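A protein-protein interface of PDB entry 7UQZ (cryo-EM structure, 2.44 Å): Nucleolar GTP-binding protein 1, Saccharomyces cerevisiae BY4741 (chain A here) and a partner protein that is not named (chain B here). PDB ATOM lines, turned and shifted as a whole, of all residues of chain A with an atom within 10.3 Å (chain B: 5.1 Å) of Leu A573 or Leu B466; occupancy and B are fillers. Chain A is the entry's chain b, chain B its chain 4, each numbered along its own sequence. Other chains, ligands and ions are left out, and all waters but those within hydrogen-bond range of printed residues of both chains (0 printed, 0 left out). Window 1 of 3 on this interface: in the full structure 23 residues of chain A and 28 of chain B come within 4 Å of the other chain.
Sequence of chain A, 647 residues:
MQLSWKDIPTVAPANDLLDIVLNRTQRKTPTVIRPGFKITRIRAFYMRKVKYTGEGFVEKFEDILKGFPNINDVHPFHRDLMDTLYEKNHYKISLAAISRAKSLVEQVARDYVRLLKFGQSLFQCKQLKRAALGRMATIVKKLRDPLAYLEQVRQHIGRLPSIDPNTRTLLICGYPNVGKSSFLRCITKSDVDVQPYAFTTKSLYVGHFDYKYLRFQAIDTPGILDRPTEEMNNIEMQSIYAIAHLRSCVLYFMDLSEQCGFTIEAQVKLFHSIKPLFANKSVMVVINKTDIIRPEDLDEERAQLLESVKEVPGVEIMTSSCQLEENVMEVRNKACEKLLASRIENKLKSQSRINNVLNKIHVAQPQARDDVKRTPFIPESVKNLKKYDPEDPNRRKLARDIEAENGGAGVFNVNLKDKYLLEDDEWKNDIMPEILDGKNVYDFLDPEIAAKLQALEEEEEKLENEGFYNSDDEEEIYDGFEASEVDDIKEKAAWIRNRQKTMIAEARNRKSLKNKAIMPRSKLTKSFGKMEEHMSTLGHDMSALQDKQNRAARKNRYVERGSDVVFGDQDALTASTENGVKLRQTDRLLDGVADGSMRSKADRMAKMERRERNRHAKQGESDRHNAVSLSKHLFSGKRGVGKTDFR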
ATOM      1  N   VAL A 566      17.140  15.557  42.646  1.00  0.00           N
ATOM      2  CA  VAL A 566      16.642  15.576  41.271  1.00  0.00           C
ATOM      3  C   VAL A 566      17.218  14.429  40.446  1.00  0.00           C
ATOM      4  O   VAL A 566      16.485  13.741  39.731  1.00  0.00           O
ATOM      5  CB  VAL A 566      16.936  16.944  40.617  1.00  0.00           C
ATOM      6  CG1 VAL A 566      16.363  16.991  39.211  1.00  0.00           C
ATOM      7  CG2 VAL A 566      16.355  18.067  41.458  1.00  0.00           C
ATOM      8  N   PHE A 567      18.531  14.203  40.518  1.00  0.00           N
ATOM      9  CA  PHE A 567      19.200  13.192  39.708  1.00  0.00           C
ATOM     10  C   PHE A 567      19.671  11.998  40.531  1.00  0.00           C
ATOM     11  O   PHE A 567      20.630  11.324  40.140  1.00  0.00           O
ATOM     12  CB  PHE A 567      20.386  13.808  38.963  1.00  0.00           C
ATOM     13  CG  PHE A 567      20.013  14.941  38.056  1.00  0.00           C
ATOM     14  CD1 PHE A 567      19.562  14.696  36.769  1.00  0.00           C
ATOM     15  CD2 PHE A 567      20.118  16.255  38.486  1.00  0.00           C
ATOM     16  CE1 PHE A 567      19.218  15.739  35.930  1.00  0.00           C
ATOM     17  CE2 PHE A 567      19.776  17.302  37.654  1.00  0.00           C
ATOM     18  CZ  PHE A 567      19.327  17.044  36.374  1.00  0.00           C
ATOM     19  N   ASP A 569      18.104   9.063  41.245  1.00  0.00           N
ATOM     20  CA  ASP A 569      17.788   7.804  40.589  1.00  0.00           C
ATOM     21  C   ASP A 569      17.729   7.909  39.072  1.00  0.00           C
ATOM     22  O   ASP A 569      17.702   6.874  38.398  1.00  0.00           O
ATOM     23  CB  ASP A 569      16.448   7.257  41.104  1.00  0.00           C
ATOM     24  CG  ASP A 569      15.334   8.278  41.015  1.00  0.00           C
ATOM     25  OD1 ASP A 569      15.590   9.461  41.323  1.00  0.00           O
ATOM     26  OD2 ASP A 569      14.205   7.902  40.633  1.00  0.00           O
ATOM     27  N   GLN A 570      17.707   9.118  38.522  1.00  0.00           N
ATOM     28  CA  GLN A 570      17.634   9.297  37.083  1.00  0.00           C
ATOM     29  C   GLN A 570      18.984   9.001  36.435  1.00  0.00           C
ATOM     30  O   GLN A 570      20.016   8.879  37.100  1.00  0.00           O
ATOM     31  CB  GLN A 570      17.180  10.716  36.743  1.00  0.00           C
ATOM     32  CG  GLN A 570      15.823  11.079  37.316  1.00  0.00           C
ATOM     33  CD  GLN A 570      15.386  12.478  36.933  1.00  0.00           C
ATOM     34  OE1 GLN A 570      16.070  13.170  36.181  1.00  0.00           O
ATOM     35  NE2 GLN A 570      14.237  12.901  37.450  1.00  0.00           N
ATOM     36  N   ASP A 571      18.965   8.886  35.111  1.00  0.00           N
ATOM     37  CA  ASP A 571      20.167   8.613  34.339  1.00  0.00           C
ATOM     38  C   ASP A 571      20.021   9.289  32.980  1.00  0.00           C
ATOM     39  O   ASP A 571      19.058  10.023  32.737  1.00  0.00           O
ATOM     40  CB  ASP A 571      20.396   7.099  34.222  1.00  0.00           C
ATOM     41  CG  ASP A 571      21.853   6.742  33.987  1.00  0.00           C
ATOM     42  OD1 ASP A 571      22.575   7.552  33.369  1.00  0.00           O
ATOM     43  OD2 ASP A 571      22.277   5.650  34.421  1.00  0.00           O
ATOM     44  N   ALA A 572      21.000   9.052  32.103  1.00  0.00           N
ATOM     45  CA  ALA A 572      20.995   9.510  30.717  1.00  0.00           C
ATOM     46  C   ALA A 572      20.897  11.026  30.599  1.00  0.00           C
ATOM     47  O   ALA A 572      21.907  11.726  30.729  1.00  0.00           O
ATOM     48  CB  ALA A 572      19.855   8.849  29.932  1.00  0.00           C
ATOM     49  N   LEU A 573      19.688  11.524  30.331  1.00  0.00           N
ATOM     50  CA  LEU A 573      19.346  12.903  29.975  1.00  0.00           C
ATOM     51  C   LEU A 573      19.936  13.320  28.633  1.00  0.00           C
ATOM     52  O   LEU A 573      19.800  14.486  28.246  1.00  0.00           O
ATOM     53  CB  LEU A 573      19.759  13.924  31.047  1.00  0.00           C
ATOM     54  CG  LEU A 573      18.792  15.094  31.244  1.00  0.00           C
ATOM     55  CD1 LEU A 573      17.462  14.585  31.779  1.00  0.00           C
ATOM     56  CD2 LEU A 573      19.383  16.158  32.158  1.00  0.00           C
ATOM     57  N   THR A 574      20.584  12.411  27.911  1.00  0.00           N
ATOM     58  CA  THR A 574      21.132  12.680  26.593  1.00  0.00           C
ATOM     59  C   THR A 574      21.093  11.388  25.791  1.00  0.00           C
ATOM     60  O   THR A 574      21.441  10.323  26.308  1.00  0.00           O
ATOM     61  CB  THR A 574      22.565  13.224  26.686  1.00  0.00           C
ATOM     62  OG1 THR A 574      22.538  14.545  27.243  1.00  0.00           O
ATOM     63  CG2 THR A 574      23.220  13.273  25.323  1.00  0.00           C
ATOM     64  N   ALA A 575      20.643  11.482  24.542  1.00  0.00           N
ATOM     65  CA  ALA A 575      20.587  10.312  23.676  1.00  0.00           C
ATOM     66  C   ALA A 575      21.990   9.788  23.398  1.00  0.00           C
ATOM     67  O   ALA A 575      22.862  10.531  22.938  1.00  0.00           O
ATOM     68  CB  ALA A 575      19.879  10.661  22.369  1.00  0.00           C
ATOM     69  N   SER A 576      22.207   8.508  23.690  1.00  0.00           N
ATOM     70  CA  SER A 576      23.488   7.881  23.398  1.00  0.00           C
ATOM     71  C   SER A 576      23.616   7.632  21.901  1.00  0.00           C
ATOM     72  O   SER A 576      22.690   7.119  21.265  1.00  0.00           O
ATOM     73  CB  SER A 576      23.628   6.572  24.171  1.00  0.00           C
ATOM     74  OG  SER A 576      22.573   5.677  23.858  1.00  0.00           O
ATOM     75  N   THR A 577      24.762   8.001  21.338  1.00  0.00           N
ATOM     76  CA  THR A 577      24.984   7.850  19.910  1.00  0.00           C
ATOM     77  C   THR A 577      25.308   6.400  19.561  1.00  0.00           C
ATOM     78  O   THR A 577      25.775   5.618  20.394  1.00  0.00           O
ATOM     79  CB  THR A 577      26.110   8.772  19.441  1.00  0.00           C
ATOM     80  OG1 THR A 577      27.280   8.545  20.236  1.00  0.00           O
ATOM     81  CG2 THR A 577      25.690  10.226  19.575  1.00  0.00           C
ATOM     82  N   LEU A 583      29.809  15.346  20.933  1.00  0.00           N
ATOM     83  CA  LEU A 583      28.748  16.226  20.446  1.00  0.00           C
ATOM     84  C   LEU A 583      29.062  16.781  19.062  1.00  0.00           C
ATOM     85  O   LEU A 583      28.192  16.804  18.184  1.00  0.00           O
ATOM     86  CB  LEU A 583      28.521  17.368  21.436  1.00  0.00           C
ATOM     87  CG  LEU A 583      27.490  18.427  21.032  1.00  0.00           C
ATOM     88  CD1 LEU A 583      26.091  17.840  21.033  1.00  0.00           C
ATOM     89  CD2 LEU A 583      27.568  19.645  21.940  1.00  0.00           C
ATOM     90  N   ILE B 258      13.643  19.548  29.541  1.00  0.00           N
ATOM     91  CA  ILE B 258      15.007  19.028  29.559  1.00  0.00           C
ATOM     92  C   ILE B 258      15.147  17.883  30.558  1.00  0.00           C
ATOM     93  O   ILE B 258      15.523  16.769  30.190  1.00  0.00           O
ATOM     94  CB  ILE B 258      16.025  20.153  29.849  1.00  0.00           C
ATOM     95  CG1 ILE B 258      15.837  21.309  28.868  1.00  0.00           C
ATOM     96  CG2 ILE B 258      17.442  19.613  29.781  1.00  0.00           C
ATOM     97  CD1 ILE B 258      16.756  22.478  29.119  1.00  0.00           C
ATOM     98  N   VAL B 259      14.846  18.139  31.827  1.00  0.00           N
ATOM     99  CA  VAL B 259      15.011  17.153  32.888  1.00  0.00           C
ATOM    100  C   VAL B 259      13.690  16.431  33.112  1.00  0.00           C
ATOM    101  O   VAL B 259      12.647  17.069  33.307  1.00  0.00           O
ATOM    102  CB  VAL B 259      15.503  17.820  34.184  1.00  0.00           C
ATOM    103  CG1 VAL B 259      15.604  16.800  35.309  1.00  0.00           C
ATOM    104  CG2 VAL B 259      16.843  18.500  33.957  1.00  0.00           C
ATOM    105  N   ALA B 260      13.730  15.102  33.078  1.00  0.00           N
ATOM    106  CA  ALA B 260      12.551  14.298  33.358  1.00  0.00           C
ATOM    107  C   ALA B 260      12.296  14.226  34.858  1.00  0.00           C
ATOM    108  O   ALA B 260      13.217  14.340  35.673  1.00  0.00           O
ATOM    109  CB  ALA B 260      12.715  12.889  32.786  1.00  0.00           C
ATOM    110  N   ASP B 363      23.789  18.414  33.856  1.00  0.00           N
ATOM    111  CA  ASP B 363      23.262  17.060  34.018  1.00  0.00           C
ATOM    112  C   ASP B 363      24.156  16.333  35.016  1.00  0.00           C
ATOM    113  O   ASP B 363      25.224  15.831  34.658  1.00  0.00           O
ATOM    114  CB  ASP B 363      23.209  16.333  32.680  1.00  0.00           C
ATOM    115  CG  ASP B 363      22.645  14.927  32.797  1.00  0.00           C
ATOM    116  OD1 ASP B 363      21.959  14.633  33.797  1.00  0.00           O
ATOM    117  OD2 ASP B 363      22.895  14.115  31.886  1.00  0.00           O
ATOM    118  N   VAL B 433      23.849  20.967  28.996  1.00  0.00           N
ATOM    119  CA  VAL B 433      22.990  21.138  27.834  1.00  0.00           C
ATOM    120  C   VAL B 433      22.465  22.568  27.825  1.00  0.00           C
ATOM    121  O   VAL B 433      22.646  23.327  28.775  1.00  0.00           O
ATOM    122  CB  VAL B 433      21.823  20.130  27.816  1.00  0.00           C
ATOM    123  CG1 VAL B 433      22.343  18.722  27.572  1.00  0.00           C
ATOM    124  CG2 VAL B 433      21.054  20.198  29.121  1.00  0.00           C
ATOM    125  N   GLU B 434      21.805  22.926  26.729  1.00  0.00           N
ATOM    126  CA  GLU B 434      21.280  24.269  26.534  1.00  0.00           C
ATOM    127  C   GLU B 434      19.779  24.296  26.784  1.00  0.00           C
ATOM    128  O   GLU B 434      19.066  23.351  26.438  1.00  0.00           O
ATOM    129  CB  GLU B 434      21.568  24.766  25.116  1.00  0.00           C
ATOM    130  CG  GLU B 434      23.040  24.902  24.783  1.00  0.00           C
ATOM    131  CD  GLU B 434      23.273  25.217  23.320  1.00  0.00           C
ATOM    132  OE1 GLU B 434      22.328  25.059  22.520  1.00  0.00           O
ATOM    133  OE2 GLU B 434      24.400  25.625  22.967  1.00  0.00           O
ATOM    134  N   SER B 464      18.982  14.422  17.436  1.00  0.00           N
ATOM    135  CA  SER B 464      18.697  15.282  18.576  1.00  0.00           C
ATOM    136  C   SER B 464      19.650  14.977  19.724  1.00  0.00           C
ATOM    137  O   SER B 464      19.885  13.813  20.061  1.00  0.00           O
ATOM    138  CB  SER B 464      17.251  15.100  19.029  1.00  0.00           C
ATOM    139  OG  SER B 464      17.012  15.784  20.246  1.00  0.00           O
ATOM    140  N   THR B 465      20.202  16.033  20.323  1.00  0.00           N
ATOM    141  CA  THR B 465      21.087  15.860  21.469  1.00  0.00           C
ATOM    142  C   THR B 465      20.305  15.527  22.734  1.00  0.00           C
ATOM    143  O   THR B 465      20.801  14.798  23.600  1.00  0.00           O
ATOM    144  CB  THR B 465      21.926  17.121  21.676  1.00  0.00           C
ATOM    145  OG1 THR B 465      21.110  18.152  22.243  1.00  0.00           O
ATOM    146  CG2 THR B 465      22.476  17.611  20.348  1.00  0.00           C
ATOM    147  N   LEU B 466      19.086  16.045  22.855  1.00  0.00           N
ATOM    148  CA  LEU B 466      18.263  15.834  24.036  1.00  0.00           C
ATOM    149  C   LEU B 466      17.255  14.718  23.797  1.00  0.00           C
ATOM    150  O   LEU B 466      16.661  14.619  22.720  1.00  0.00           O
ATOM    151  CB  LEU B 466      17.537  17.124  24.424  1.00  0.00           C
ATOM    152  CG  LEU B 466      18.174  17.976  25.525  1.00  0.00           C
ATOM    153  CD1 LEU B 466      18.302  17.173  26.810  1.00  0.00           C
ATOM    154  CD2 LEU B 466      19.528  18.511  25.093  1.00  0.00           C
ATOM    155  N   THR B 467      17.069  13.877  24.816  1.00  0.00           N
ATOM    156  CA  THR B 467      16.196  12.715  24.681  1.00  0.00           C
ATOM    157  C   THR B 467      14.725  13.118  24.651  1.00  0.00           C
ATOM    158  O   THR B 467      13.954  12.621  23.819  1.00  0.00           O
ATOM    159  CB  THR B 467      16.455  11.733  25.825  1.00  0.00           C
ATOM    160  OG1 THR B 467      17.843  11.377  25.850  1.00  0.00           O
ATOM    161  CG2 THR B 467      15.619  10.472  25.652  1.00  0.00           C
ATOM    162  N   LEU B 468      14.316  14.011  25.555  1.00  0.00           N
ATOM    163  CA  LEU B 468      12.893  14.313  25.714  1.00  0.00           C
ATOM    164  C   LEU B 468      12.264  14.967  24.485  1.00  0.00           C
ATOM    165  O   LEU B 468      11.187  14.511  24.063  1.00  0.00           O
ATOM    166  CB  LEU B 468      12.678  15.149  26.984  1.00  0.00           C
ATOM    167  CG  LEU B 468      12.317  14.412  28.279  1.00  0.00           C
ATOM    168  CD1 LEU B 468      13.389  13.408  28.674  1.00  0.00           C
ATOM    169  CD2 LEU B 468      12.077  15.401  29.410  1.00  0.00           C
ATOM    170  N   PRO B 469      12.843  16.007  23.861  1.00  0.00           N
ATOM    171  CA  PRO B 469      12.242  16.510  22.615  1.00  0.00           C
ATOM    172  C   PRO B 469      12.537  15.645  21.403  1.00  0.00           C
ATOM    173  O   PRO B 469      11.813  15.751  20.402  1.00  0.00           O
ATOM    174  CB  PRO B 469      12.867  17.907  22.453  1.00  0.00           C
ATOM    175  CG  PRO B 469      13.509  18.214  23.762  1.00  0.00           C
ATOM    176  CD  PRO B 469      13.936  16.894  24.295  1.00  0.00           C
ATOM    177  N   GLY B 470      13.574  14.808  21.453  1.00  0.00           N
ATOM    178  CA  GLY B 470      13.901  13.976  20.308  1.00  0.00           C
ATOM    179  C   GLY B 470      12.858  12.910  20.030  1.00  0.00           C
ATOM    180  O   GLY B 470      12.546  12.621  18.872  1.00  0.00           O
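Of the 13 printed residues of chain B, 8 touch a printed residue of chain A. Hydrophobic or aromatic side chains of chain A that line the printed part of chain B: Val A566, Phe A567, Leu A573, Ala A575 and Leu A583.
The backbone carbonyl oxygen of Ala A572 sits close to the side-chain carboxylate of Asp B363 (2.8 Å). The side-chain amide nitrogen (NE2) of Gln A570 is in hydrogen-bond range of the backbone carbonyl oxygen (O) of Ala B260 (2.5 Å). OG1 of Thr B467 is in hydrogen-bond range of N of Ala A575, 3.1 Å away. The backbone NH of Ala A575 sits at hydrogen-bond distance from the backbone carbonyl oxygen of Thr B465.
Val A566 touches Val B259 (CG1 to CG1, 3.98 Å). CG2 of Val B259 touches CZ of Phe A567, at 3.8 Å. OD1 of Asp B363 touches CE1 of Phe A567 (3.6 Å). Gln A570 touches Val B259. Leu A573 touches Ala B260. Asp B363 touches Leu A573. O of Leu A573 touches CD1 of Leu B466, 3.4 Å away. Leu A573 touches Thr B467. Thr A574 touches Thr B467. CB of Ala A575 touches O of Ser B464 (3.9 Å).
OG of Ser B464 is in hydrogen-bond range of O of Leu B466, at 2.8 Å. The backbone carbonyl oxygen of Val A566 sits close to the side-chain amide nitrogen of Gln A570 (3.3 Å).
Of the printed residues of chain B, Leu A573 touches Ile B258 (3.3 Å), Val B259 (3.7 Å), Ala B260 (3.99 Å), Asp B363 (3.3 Å), Leu B466 (3.4 Å) and Thr B467 (3.99 Å). Leu B466 touches just one residue of chain A: Leu A573 (3.4 Å). Printed residues of chain A within 4 Å of Ile B258: Leu A573. Of the printed residues of chain A, Val B259 touches Val A566 (3.98 Å), Phe A567 (3.8 Å), Gln A570 (3.8 Å) and Leu A573 (3.7 Å). Of chain A, only Ala A575 (3.9 Å) comes within 4 Å of Ser B464. No residue of chain A comes within 4 Å of Pro B469. No residue of chain A comes within 4 Å of Gly B470. Of the printed residues of chain A, Asp B363 touches Phe A567 (3.6 Å), Ala A572 (2.8 Å) and Leu A573 (3.3 Å). Printed residues of chain B within 4 Å of Gln A570: Val B259 (3.8 Å) and Ala B260 (2.5 Å). Of the printed residues of chain B, Thr A574 touches Thr B465 and Thr B467. Glu B434 touches none of the printed residues of chain A. Asp A571 touches none of the printed residues of chain B. The nearest residue of chain A that does not touch Leu B466 is Ala A575 (4.7 Å). The nearest printed residue of chain B that does not touch Thr A574 is Val B433 (4.2 Å).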
